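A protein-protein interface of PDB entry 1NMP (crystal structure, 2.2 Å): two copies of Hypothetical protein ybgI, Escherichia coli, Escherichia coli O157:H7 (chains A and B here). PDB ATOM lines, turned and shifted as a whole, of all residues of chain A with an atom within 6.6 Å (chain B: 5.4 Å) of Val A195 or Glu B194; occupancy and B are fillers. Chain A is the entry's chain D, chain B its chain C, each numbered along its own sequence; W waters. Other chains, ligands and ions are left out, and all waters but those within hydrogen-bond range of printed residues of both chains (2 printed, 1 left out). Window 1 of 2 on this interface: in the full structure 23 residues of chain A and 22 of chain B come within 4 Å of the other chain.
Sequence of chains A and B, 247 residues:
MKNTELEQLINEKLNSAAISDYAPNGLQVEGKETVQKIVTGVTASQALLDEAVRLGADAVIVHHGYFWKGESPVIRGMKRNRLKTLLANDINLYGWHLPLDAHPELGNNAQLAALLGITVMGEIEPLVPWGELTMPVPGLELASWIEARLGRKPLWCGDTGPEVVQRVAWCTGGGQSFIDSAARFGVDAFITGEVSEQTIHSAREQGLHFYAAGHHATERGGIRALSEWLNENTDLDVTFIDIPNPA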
ATOM      1  N   LEU A 155       2.241  14.074   6.286  1.00  0.00           N
ATOM      2  CA  LEU A 155       2.132  14.341   4.833  1.00  0.00           C
ATOM      3  C   LEU A 155       3.151  15.487   4.615  1.00  0.00           C
ATOM      4  O   LEU A 155       3.099  16.497   5.350  1.00  0.00           O
ATOM      5  CB  LEU A 155       0.731  14.890   4.512  1.00  0.00           C
ATOM      6  CG  LEU A 155       0.578  15.628   3.153  1.00  0.00           C
ATOM      7  CD1 LEU A 155       0.765  14.630   2.061  1.00  0.00           C
ATOM      8  CD2 LEU A 155      -0.807  16.287   3.034  1.00  0.00           C
ATOM      9  N   GLY A 173      -3.166  21.019  15.589  1.00  0.00           N
ATOM     10  CA  GLY A 173      -4.542  20.727  15.311  1.00  0.00           C
ATOM     11  C   GLY A 173      -4.977  21.119  13.943  1.00  0.00           C
ATOM     12  O   GLY A 173      -4.256  20.855  12.963  1.00  0.00           O
ATOM     13  N   GLN A 176      -4.592  24.545   9.296  1.00  0.00           N
ATOM     14  CA  GLN A 176      -4.183  24.694   7.895  1.00  0.00           C
ATOM     15  C   GLN A 176      -4.478  26.004   7.322  1.00  0.00           C
ATOM     16  O   GLN A 176      -3.838  26.387   6.326  1.00  0.00           O
ATOM     17  CB  GLN A 176      -4.927  23.855   6.892  1.00  0.00           C
ATOM     18  CG  GLN A 176      -5.305  22.498   7.192  1.00  0.00           C
ATOM     19  CD  GLN A 176      -6.465  22.391   8.140  1.00  0.00           C
ATOM     20  OE1 GLN A 176      -6.236  22.546   9.334  1.00  0.00           O
ATOM     21  NE2 GLN A 176      -7.695  22.034   7.648  1.00  0.00           N
ATOM     22  N   THR A 192       1.320  21.988  10.719  1.00  0.00           N
ATOM     23  CA  THR A 192       0.081  22.007  11.460  1.00  0.00           C
ATOM     24  C   THR A 192      -0.425  20.555  11.576  1.00  0.00           C
ATOM     25  O   THR A 192       0.303  19.620  11.189  1.00  0.00           O
ATOM     26  CB  THR A 192      -0.941  22.847  10.777  1.00  0.00           C
ATOM     27  OG1 THR A 192      -2.017  23.003  11.714  1.00  0.00           O
ATOM     28  CG2 THR A 192      -1.503  22.150   9.488  1.00  0.00           C
ATOM     29  N   GLY A 193      -1.650  20.336  12.059  1.00  0.00           N
ATOM     30  CA  GLY A 193      -2.116  18.964  12.133  1.00  0.00           C
ATOM     31  C   GLY A 193      -2.857  18.396  10.923  1.00  0.00           C
ATOM     32  O   GLY A 193      -2.479  17.334  10.377  1.00  0.00           O
ATOM     33  N   GLU A 194      -3.919  19.056  10.473  1.00  0.00           N
ATOM     34  CA  GLU A 194      -4.707  18.527   9.341  1.00  0.00           C
ATOM     35  C   GLU A 194      -4.297  19.179   8.032  1.00  0.00           C
ATOM     36  O   GLU A 194      -3.436  20.035   8.005  1.00  0.00           O
ATOM     37  CB  GLU A 194      -6.210  18.835   9.538  1.00  0.00           C
ATOM     38  CG  GLU A 194      -6.833  18.230  10.849  1.00  0.00           C
ATOM     39  CD  GLU A 194      -8.327  18.493  11.005  1.00  0.00           C
ATOM     40  OE1 GLU A 194      -8.961  19.059  10.026  1.00  0.00           O
ATOM     41  OE2 GLU A 194      -8.865  18.142  12.118  1.00  0.00           O
ATOM     42  N   VAL A 195      -4.938  18.767   6.938  1.00  0.00           N
ATOM     43  CA  VAL A 195      -4.692  19.381   5.657  1.00  0.00           C
ATOM     44  C   VAL A 195      -6.041  19.485   4.938  1.00  0.00           C
ATOM     45  O   VAL A 195      -7.019  18.778   5.276  1.00  0.00           O
ATOM     46  CB  VAL A 195      -3.695  18.576   4.765  1.00  0.00           C
ATOM     47  CG1 VAL A 195      -4.325  17.200   4.260  1.00  0.00           C
ATOM     48  CG2 VAL A 195      -3.349  19.455   3.578  1.00  0.00           C
ATOM     49  N   SER A 196      -6.087  20.408   3.980  1.00  0.00           N
ATOM     50  CA  SER A 196      -7.268  20.636   3.170  1.00  0.00           C
ATOM     51  C   SER A 196      -6.738  20.754   1.750  1.00  0.00           C
ATOM     52  O   SER A 196      -5.540  20.958   1.564  1.00  0.00           O
ATOM     53  CB  SER A 196      -7.960  21.965   3.514  1.00  0.00           C
ATOM     54  OG  SER A 196      -8.580  21.934   4.777  1.00  0.00           O
ATOM     55  N   GLU A 197      -7.649  20.716   0.776  1.00  0.00           N
ATOM     56  CA  GLU A 197      -7.322  20.814  -0.638  1.00  0.00           C
ATOM     57  C   GLU A 197      -6.577  22.068  -0.994  1.00  0.00           C
ATOM     58  O   GLU A 197      -5.616  21.974  -1.726  1.00  0.00           O
ATOM     59  CB  GLU A 197      -8.593  20.812  -1.514  1.00  0.00           C
ATOM     60  CG  GLU A 197      -8.310  20.648  -3.056  1.00  0.00           C
ATOM     61  CD  GLU A 197      -8.192  21.947  -3.807  1.00  0.00           C
ATOM     62  OE1 GLU A 197      -8.529  23.056  -3.240  1.00  0.00           O
ATOM     63  OE2 GLU A 197      -7.765  21.875  -5.007  1.00  0.00           O
ATOM     64  N   GLN A 198      -7.047  23.246  -0.569  1.00  0.00           N
ATOM     65  CA  GLN A 198      -6.346  24.502  -0.937  1.00  0.00           C
ATOM     66  C   GLN A 198      -4.955  24.633  -0.275  1.00  0.00           C
ATOM     67  O   GLN A 198      -4.072  25.390  -0.733  1.00  0.00           O
ATOM     68  CB  GLN A 198      -7.181  25.708  -0.504  1.00  0.00           C
ATOM     69  CG  GLN A 198      -7.517  25.675   1.043  1.00  0.00           C
ATOM     70  CD  GLN A 198      -8.849  24.949   1.384  1.00  0.00           C
ATOM     71  OE1 GLN A 198      -9.155  23.821   0.877  1.00  0.00           O
ATOM     72  NE2 GLN A 198      -9.655  25.591   2.253  1.00  0.00           N
ATOM     73  N   THR A 199      -4.731  23.911   0.821  1.00  0.00           N
ATOM     74  CA  THR A 199      -3.451  24.036   1.499  1.00  0.00           C
ATOM     75  C   THR A 199      -2.290  23.609   0.641  1.00  0.00           C
ATOM     76  O   THR A 199      -1.152  24.118   0.791  1.00  0.00           O
ATOM     77  CB  THR A 199      -3.426  23.167   2.754  1.00  0.00           C
ATOM     78  OG1 THR A 199      -4.654  23.377   3.480  1.00  0.00           O
ATOM     79  CG2 THR A 199      -2.197  23.524   3.676  1.00  0.00           C
ATOM     80  N   ILE A 200      -2.511  22.653  -0.248  1.00  0.00           N
ATOM     81  CA  ILE A 200      -1.392  22.131  -1.057  1.00  0.00           C
ATOM     82  C   ILE A 200      -1.023  23.183  -2.076  1.00  0.00           C
ATOM     83  O   ILE A 200       0.149  23.307  -2.386  1.00  0.00           O
ATOM     84  CB  ILE A 200      -1.806  20.832  -1.786  1.00  0.00           C
ATOM     85  CG1 ILE A 200      -1.938  19.711  -0.760  1.00  0.00           C
ATOM     86  CG2 ILE A 200      -0.718  20.395  -2.802  1.00  0.00           C
ATOM     87  CD1 ILE A 200      -0.702  19.509   0.075  1.00  0.00           C
ATOM     88  N   PHE A 210       5.490  22.185   3.515  1.00  0.00           N
ATOM     89  CA  PHE A 210       4.321  22.077   4.350  1.00  0.00           C
ATOM     90  C   PHE A 210       4.210  20.679   5.025  1.00  0.00           C
ATOM     91  O   PHE A 210       4.529  19.686   4.428  1.00  0.00           O
ATOM     92  CB  PHE A 210       3.083  22.372   3.506  1.00  0.00           C
ATOM     93  CG  PHE A 210       1.829  22.003   4.205  1.00  0.00           C
ATOM     94  CD1 PHE A 210       1.386  22.745   5.289  1.00  0.00           C
ATOM     95  CD2 PHE A 210       1.137  20.830   3.852  1.00  0.00           C
ATOM     96  CE1 PHE A 210       0.272  22.319   6.020  1.00  0.00           C
ATOM     97  CE2 PHE A 210       0.003  20.403   4.587  1.00  0.00           C
ATOM     98  CZ  PHE A 210      -0.425  21.149   5.671  1.00  0.00           C
ATOM     99  N   ALA A 212       1.475  18.155   7.351  1.00  0.00           N
ATOM    100  CA  ALA A 212       0.203  17.966   8.082  1.00  0.00           C
ATOM    101  C   ALA A 212       0.699  16.842   8.976  1.00  0.00           C
ATOM    102  O   ALA A 212       0.895  15.686   8.505  1.00  0.00           O
ATOM    103  CB  ALA A 212      -0.936  17.402   7.161  1.00  0.00           C
ATOM    104  N   GLY B 173     -15.158  15.660  -1.635  1.00  0.00           N
ATOM    105  CA  GLY B 173     -14.513  16.873  -1.140  1.00  0.00           C
ATOM    106  C   GLY B 173     -14.477  16.961   0.371  1.00  0.00           C
ATOM    107  O   GLY B 173     -14.260  15.970   1.057  1.00  0.00           O
ATOM    108  N   GLY B 174     -14.732  18.134   0.920  1.00  0.00           N
ATOM    109  CA  GLY B 174     -14.687  18.270   2.380  1.00  0.00           C
ATOM    110  C   GLY B 174     -16.046  18.017   3.049  1.00  0.00           C
ATOM    111  O   GLY B 174     -16.702  18.906   3.621  1.00  0.00           O
ATOM    112  N   GLY B 175     -16.494  16.784   3.013  1.00  0.00           N
ATOM    113  CA  GLY B 175     -17.771  16.539   3.626  1.00  0.00           C
ATOM    114  C   GLY B 175     -17.674  15.644   4.834  1.00  0.00           C
ATOM    115  O   GLY B 175     -18.659  14.924   5.107  1.00  0.00           O
ATOM    116  N   GLN B 176     -16.554  15.712   5.588  1.00  0.00           N
ATOM    117  CA  GLN B 176     -16.407  14.808   6.745  1.00  0.00           C
ATOM    118  C   GLN B 176     -17.472  15.131   7.754  1.00  0.00           C
ATOM    119  O   GLN B 176     -17.765  14.317   8.634  1.00  0.00           O
ATOM    120  CB  GLN B 176     -15.127  15.014   7.563  1.00  0.00           C
ATOM    121  CG  GLN B 176     -13.864  15.378   6.896  1.00  0.00           C
ATOM    122  CD  GLN B 176     -13.795  16.811   6.379  1.00  0.00           C
ATOM    123  OE1 GLN B 176     -14.574  17.148   5.524  1.00  0.00           O
ATOM    124  NE2 GLN B 176     -12.822  17.631   6.854  1.00  0.00           N
ATOM    125  N   THR B 192     -15.901  10.124   2.077  1.00  0.00           N
ATOM    126  CA  THR B 192     -15.841  11.535   1.736  1.00  0.00           C
ATOM    127  C   THR B 192     -14.435  11.783   1.212  1.00  0.00           C
ATOM    128  O   THR B 192     -13.772  10.843   0.758  1.00  0.00           O
ATOM    129  CB  THR B 192     -16.171  12.473   2.917  1.00  0.00           C
ATOM    130  OG1 THR B 192     -16.304  13.782   2.376  1.00  0.00           O
ATOM    131  CG2 THR B 192     -15.069  12.535   4.004  1.00  0.00           C
ATOM    132  N   GLY B 193     -13.967  13.023   1.217  1.00  0.00           N
ATOM    133  CA  GLY B 193     -12.616  13.285   0.712  1.00  0.00           C
ATOM    134  C   GLY B 193     -11.625  13.616   1.817  1.00  0.00           C
ATOM    135  O   GLY B 193     -10.592  12.999   1.907  1.00  0.00           O
ATOM    136  N   GLU B 194     -11.917  14.591   2.661  1.00  0.00           N
ATOM    137  CA  GLU B 194     -10.996  14.939   3.740  1.00  0.00           C
ATOM    138  C   GLU B 194     -11.387  14.274   5.072  1.00  0.00           C
ATOM    139  O   GLU B 194     -12.451  13.598   5.152  1.00  0.00           O
ATOM    140  CB  GLU B 194     -10.982  16.467   3.874  1.00  0.00           C
ATOM    141  CG  GLU B 194     -10.504  17.217   2.612  1.00  0.00           C
ATOM    142  CD  GLU B 194     -10.333  18.779   2.836  1.00  0.00           C
ATOM    143  OE1 GLU B 194     -10.570  19.269   3.985  1.00  0.00           O
ATOM    144  OE2 GLU B 194      -9.961  19.482   1.841  1.00  0.00           O
ATOM    145  N   VAL B 195     -10.562  14.455   6.119  1.00  0.00           N
ATOM    146  CA  VAL B 195     -10.850  13.882   7.458  1.00  0.00           C
ATOM    147  C   VAL B 195     -10.432  14.918   8.489  1.00  0.00           C
ATOM    148  O   VAL B 195      -9.570  15.782   8.213  1.00  0.00           O
ATOM    149  CB  VAL B 195     -10.112  12.495   7.786  1.00  0.00           C
ATOM    150  CG1 VAL B 195      -8.612  12.620   7.878  1.00  0.00           C
ATOM    151  CG2 VAL B 195     -10.637  11.928   9.126  1.00  0.00           C
ATOM    152  N   SER B 196     -11.131  14.872   9.638  1.00  0.00           N
ATOM    153  CA  SER B 196     -10.897  15.758  10.771  1.00  0.00           C
ATOM    154  C   SER B 196     -10.839  14.925  12.028  1.00  0.00           C
ATOM    155  O   SER B 196     -11.337  13.799  12.042  1.00  0.00           O
ATOM    156  CB  SER B 196     -12.014  16.805  10.921  1.00  0.00           C
ATOM    157  OG  SER B 196     -11.949  17.702   9.841  1.00  0.00           O
ATOM    158  N   PHE B 210     -15.412   4.127   7.900  1.00  0.00           N
ATOM    159  CA  PHE B 210     -15.219   5.457   7.384  1.00  0.00           C
ATOM    160  C   PHE B 210     -14.057   5.503   6.408  1.00  0.00           C
ATOM    161  O   PHE B 210     -13.053   4.885   6.637  1.00  0.00           O
ATOM    162  CB  PHE B 210     -14.953   6.456   8.510  1.00  0.00           C
ATOM    163  CG  PHE B 210     -14.591   7.789   7.985  1.00  0.00           C
ATOM    164  CD1 PHE B 210     -15.558   8.588   7.339  1.00  0.00           C
ATOM    165  CD2 PHE B 210     -13.270   8.260   8.083  1.00  0.00           C
ATOM    166  CE1 PHE B 210     -15.207   9.841   6.802  1.00  0.00           C
ATOM    167  CE2 PHE B 210     -12.944   9.498   7.544  1.00  0.00           C
ATOM    168  CZ  PHE B 210     -13.924  10.294   6.903  1.00  0.00           C
ATOM    169  N   ALA B 212     -11.622   8.328   4.051  1.00  0.00           N
ATOM    170  CA  ALA B 212     -11.241   9.666   3.662  1.00  0.00           C
ATOM    171  C   ALA B 212     -10.480   9.338   2.389  1.00  0.00           C
ATOM    172  O   ALA B 212      -9.353   8.903   2.449  1.00  0.00           O
ATOM    173  CB  ALA B 212     -10.279  10.278   4.702  1.00  0.00           C
ATOM    174  N   ALA B 213     -11.109   9.504   1.229  1.00  0.00           N
ATOM    175  CA  ALA B 213     -10.474   9.126  -0.039  1.00  0.00           C
ATOM    176  C   ALA B 213      -9.756  10.204  -0.888  1.00  0.00           C
ATOM    177  O   ALA B 213      -9.321   9.898  -2.078  1.00  0.00           O
ATOM    178  CB  ALA B 213     -11.593   8.394  -0.982  1.00  0.00           C
ATOM    179  N   GLY B 214      -9.719  11.471  -0.397  1.00  0.00           N
ATOM    180  CA  GLY B 214      -8.996  12.530  -1.127  1.00  0.00           C
ATOM    181  C   GLY B 214      -9.890  13.645  -1.611  1.00  0.00           C
ATOM    182  O   GLY B 214     -10.827  13.413  -2.389  1.00  0.00           O
ATOM    183  N   HIS B 215      -9.641  14.873  -1.186  1.00  0.00           N
ATOM    184  CA  HIS B 215     -10.508  15.919  -1.631  1.00  0.00           C
ATOM    185  C   HIS B 215     -10.378  15.959  -3.140  1.00  0.00           C
ATOM    186  O   HIS B 215     -11.350  15.830  -3.881  1.00  0.00           O
ATOM    187  CB  HIS B 215     -10.075  17.252  -1.056  1.00  0.00           C
ATOM    188  CG  HIS B 215     -11.072  18.359  -1.257  1.00  0.00           C
ATOM    189  ND1 HIS B 215     -11.553  19.110  -0.202  1.00  0.00           N
ATOM    190  CD2 HIS B 215     -11.677  18.857  -2.371  1.00  0.00           C
ATOM    191  CE1 HIS B 215     -12.413  20.026  -0.646  1.00  0.00           C
ATOM    192  NE2 HIS B 215     -12.511  19.892  -1.961  1.00  0.00           N
ATOM    193  N   ALA B 247      -4.004  16.053  -1.020  1.00  0.00           N
ATOM    194  CA  ALA B 247      -5.172  16.269  -0.154  1.00  0.00           C
ATOM    195  C   ALA B 247      -6.561  15.937  -0.727  1.00  0.00           C
ATOM    196  O   ALA B 247      -7.506  15.597   0.067  1.00  0.00           O
ATOM    197  CB  ALA B 247      -5.164  17.707   0.330  1.00  0.00           C
ATOM    198  OXT ALA B 247      -6.694  16.054  -1.956  1.00  0.00           O
HETATM  199  O   HOH W   1      -8.164  15.875   5.212  1.00  0.00           O
HETATM  200  O   HOH W   2      -6.759  16.291   7.574  1.00  0.00           O
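The side-chain amide nitrogen (NE2) of Gln A176 sits at hydrogen-bond distance from the side-chain hydroxyl (OG) of Ser A196 (3.0 Å). The backbone NH (N) of His B215 sits at hydrogen-bond distance from the chain-end carboxylate (O) of Ala B247 (2.6 Å). The side-chain carboxylate of Glu B194 sits at hydrogen-bond distance from a ring nitrogen (ND1) of His B215 (2.6 Å). The backbone NH (N) of Glu A194 is in hydrogen-bond range of the backbone carbonyl oxygen (O) of Gly A173 (3.1 Å). The side-chain hydroxyl of Ser B196 sits at hydrogen-bond distance from the side-chain amide nitrogen of Gln B176, 3.1 Å away. The backbone carbonyl oxygen (O) of Gly B173 is in hydrogen-bond range of the backbone NH (N) of Glu B194.
OE2 of Glu B194 is in hydrogen-bond range of N of Glu A197 (2.8 Å). OG of Ser A196 is in hydrogen-bond range of OE1 of Glu B194 (3.4 Å). OE1 of Glu A194 is in hydrogen-bond range of OG of Ser B196 (3.3 Å).
Hydrophobic or aromatic side chains of chain B that line the printed part of chain A: His B215 and Ala B247.
Glu A194 touches Val B195, and with the chains exchanged Val A195 touches Glu B194. Glu A194 touches Ser B196, and with the chains exchanged Ser A196 touches Glu B194.
Of chain B, only Glu B194 (3.8 Å) comes within 4 Å of Val A195. Of chain A, only Val A195, Ser A196 and Glu A197 come within 4 Å of Glu B194. Of the printed residues of chain B, Ile A200 touches Ala B247 (3.95 Å). Printed residues of chain B within 4 Å of Ser A196: Glu B194 and Ala B247. Of the printed residues of chain A, Val B195 touches Glu A194. Phe B210 touches none of the printed residues of chain A. The nearest residue of chain B that does not touch Val A195 is Ala B247 (4.1 Å). The nearest residue of chain A that does not touch Glu B194 is Gln A198 (4.5 Å). The nearest printed residue of chain B that does not touch Glu A194 is Gln B176 (5.2 Å).
OE1 of Glu A194 touches O of Val B195, 3.8 Å away. Val A195 touches Glu B194. Ser A196 touches Ala B247 (O to CB, 3.5 Å). Glu A197 touches His B215. Glu A197 touches Ala B247. CG1 of Ile A200 touches CB of Ala B247, 3.95 Å away.
Water W2 lies within hydrogen-bond range of O of Val B195 (2.9 Å) and N of Val A195 (3.1 Å). Water W1 lies within hydrogen-bond range of N of Val B195 and O of Val A195.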
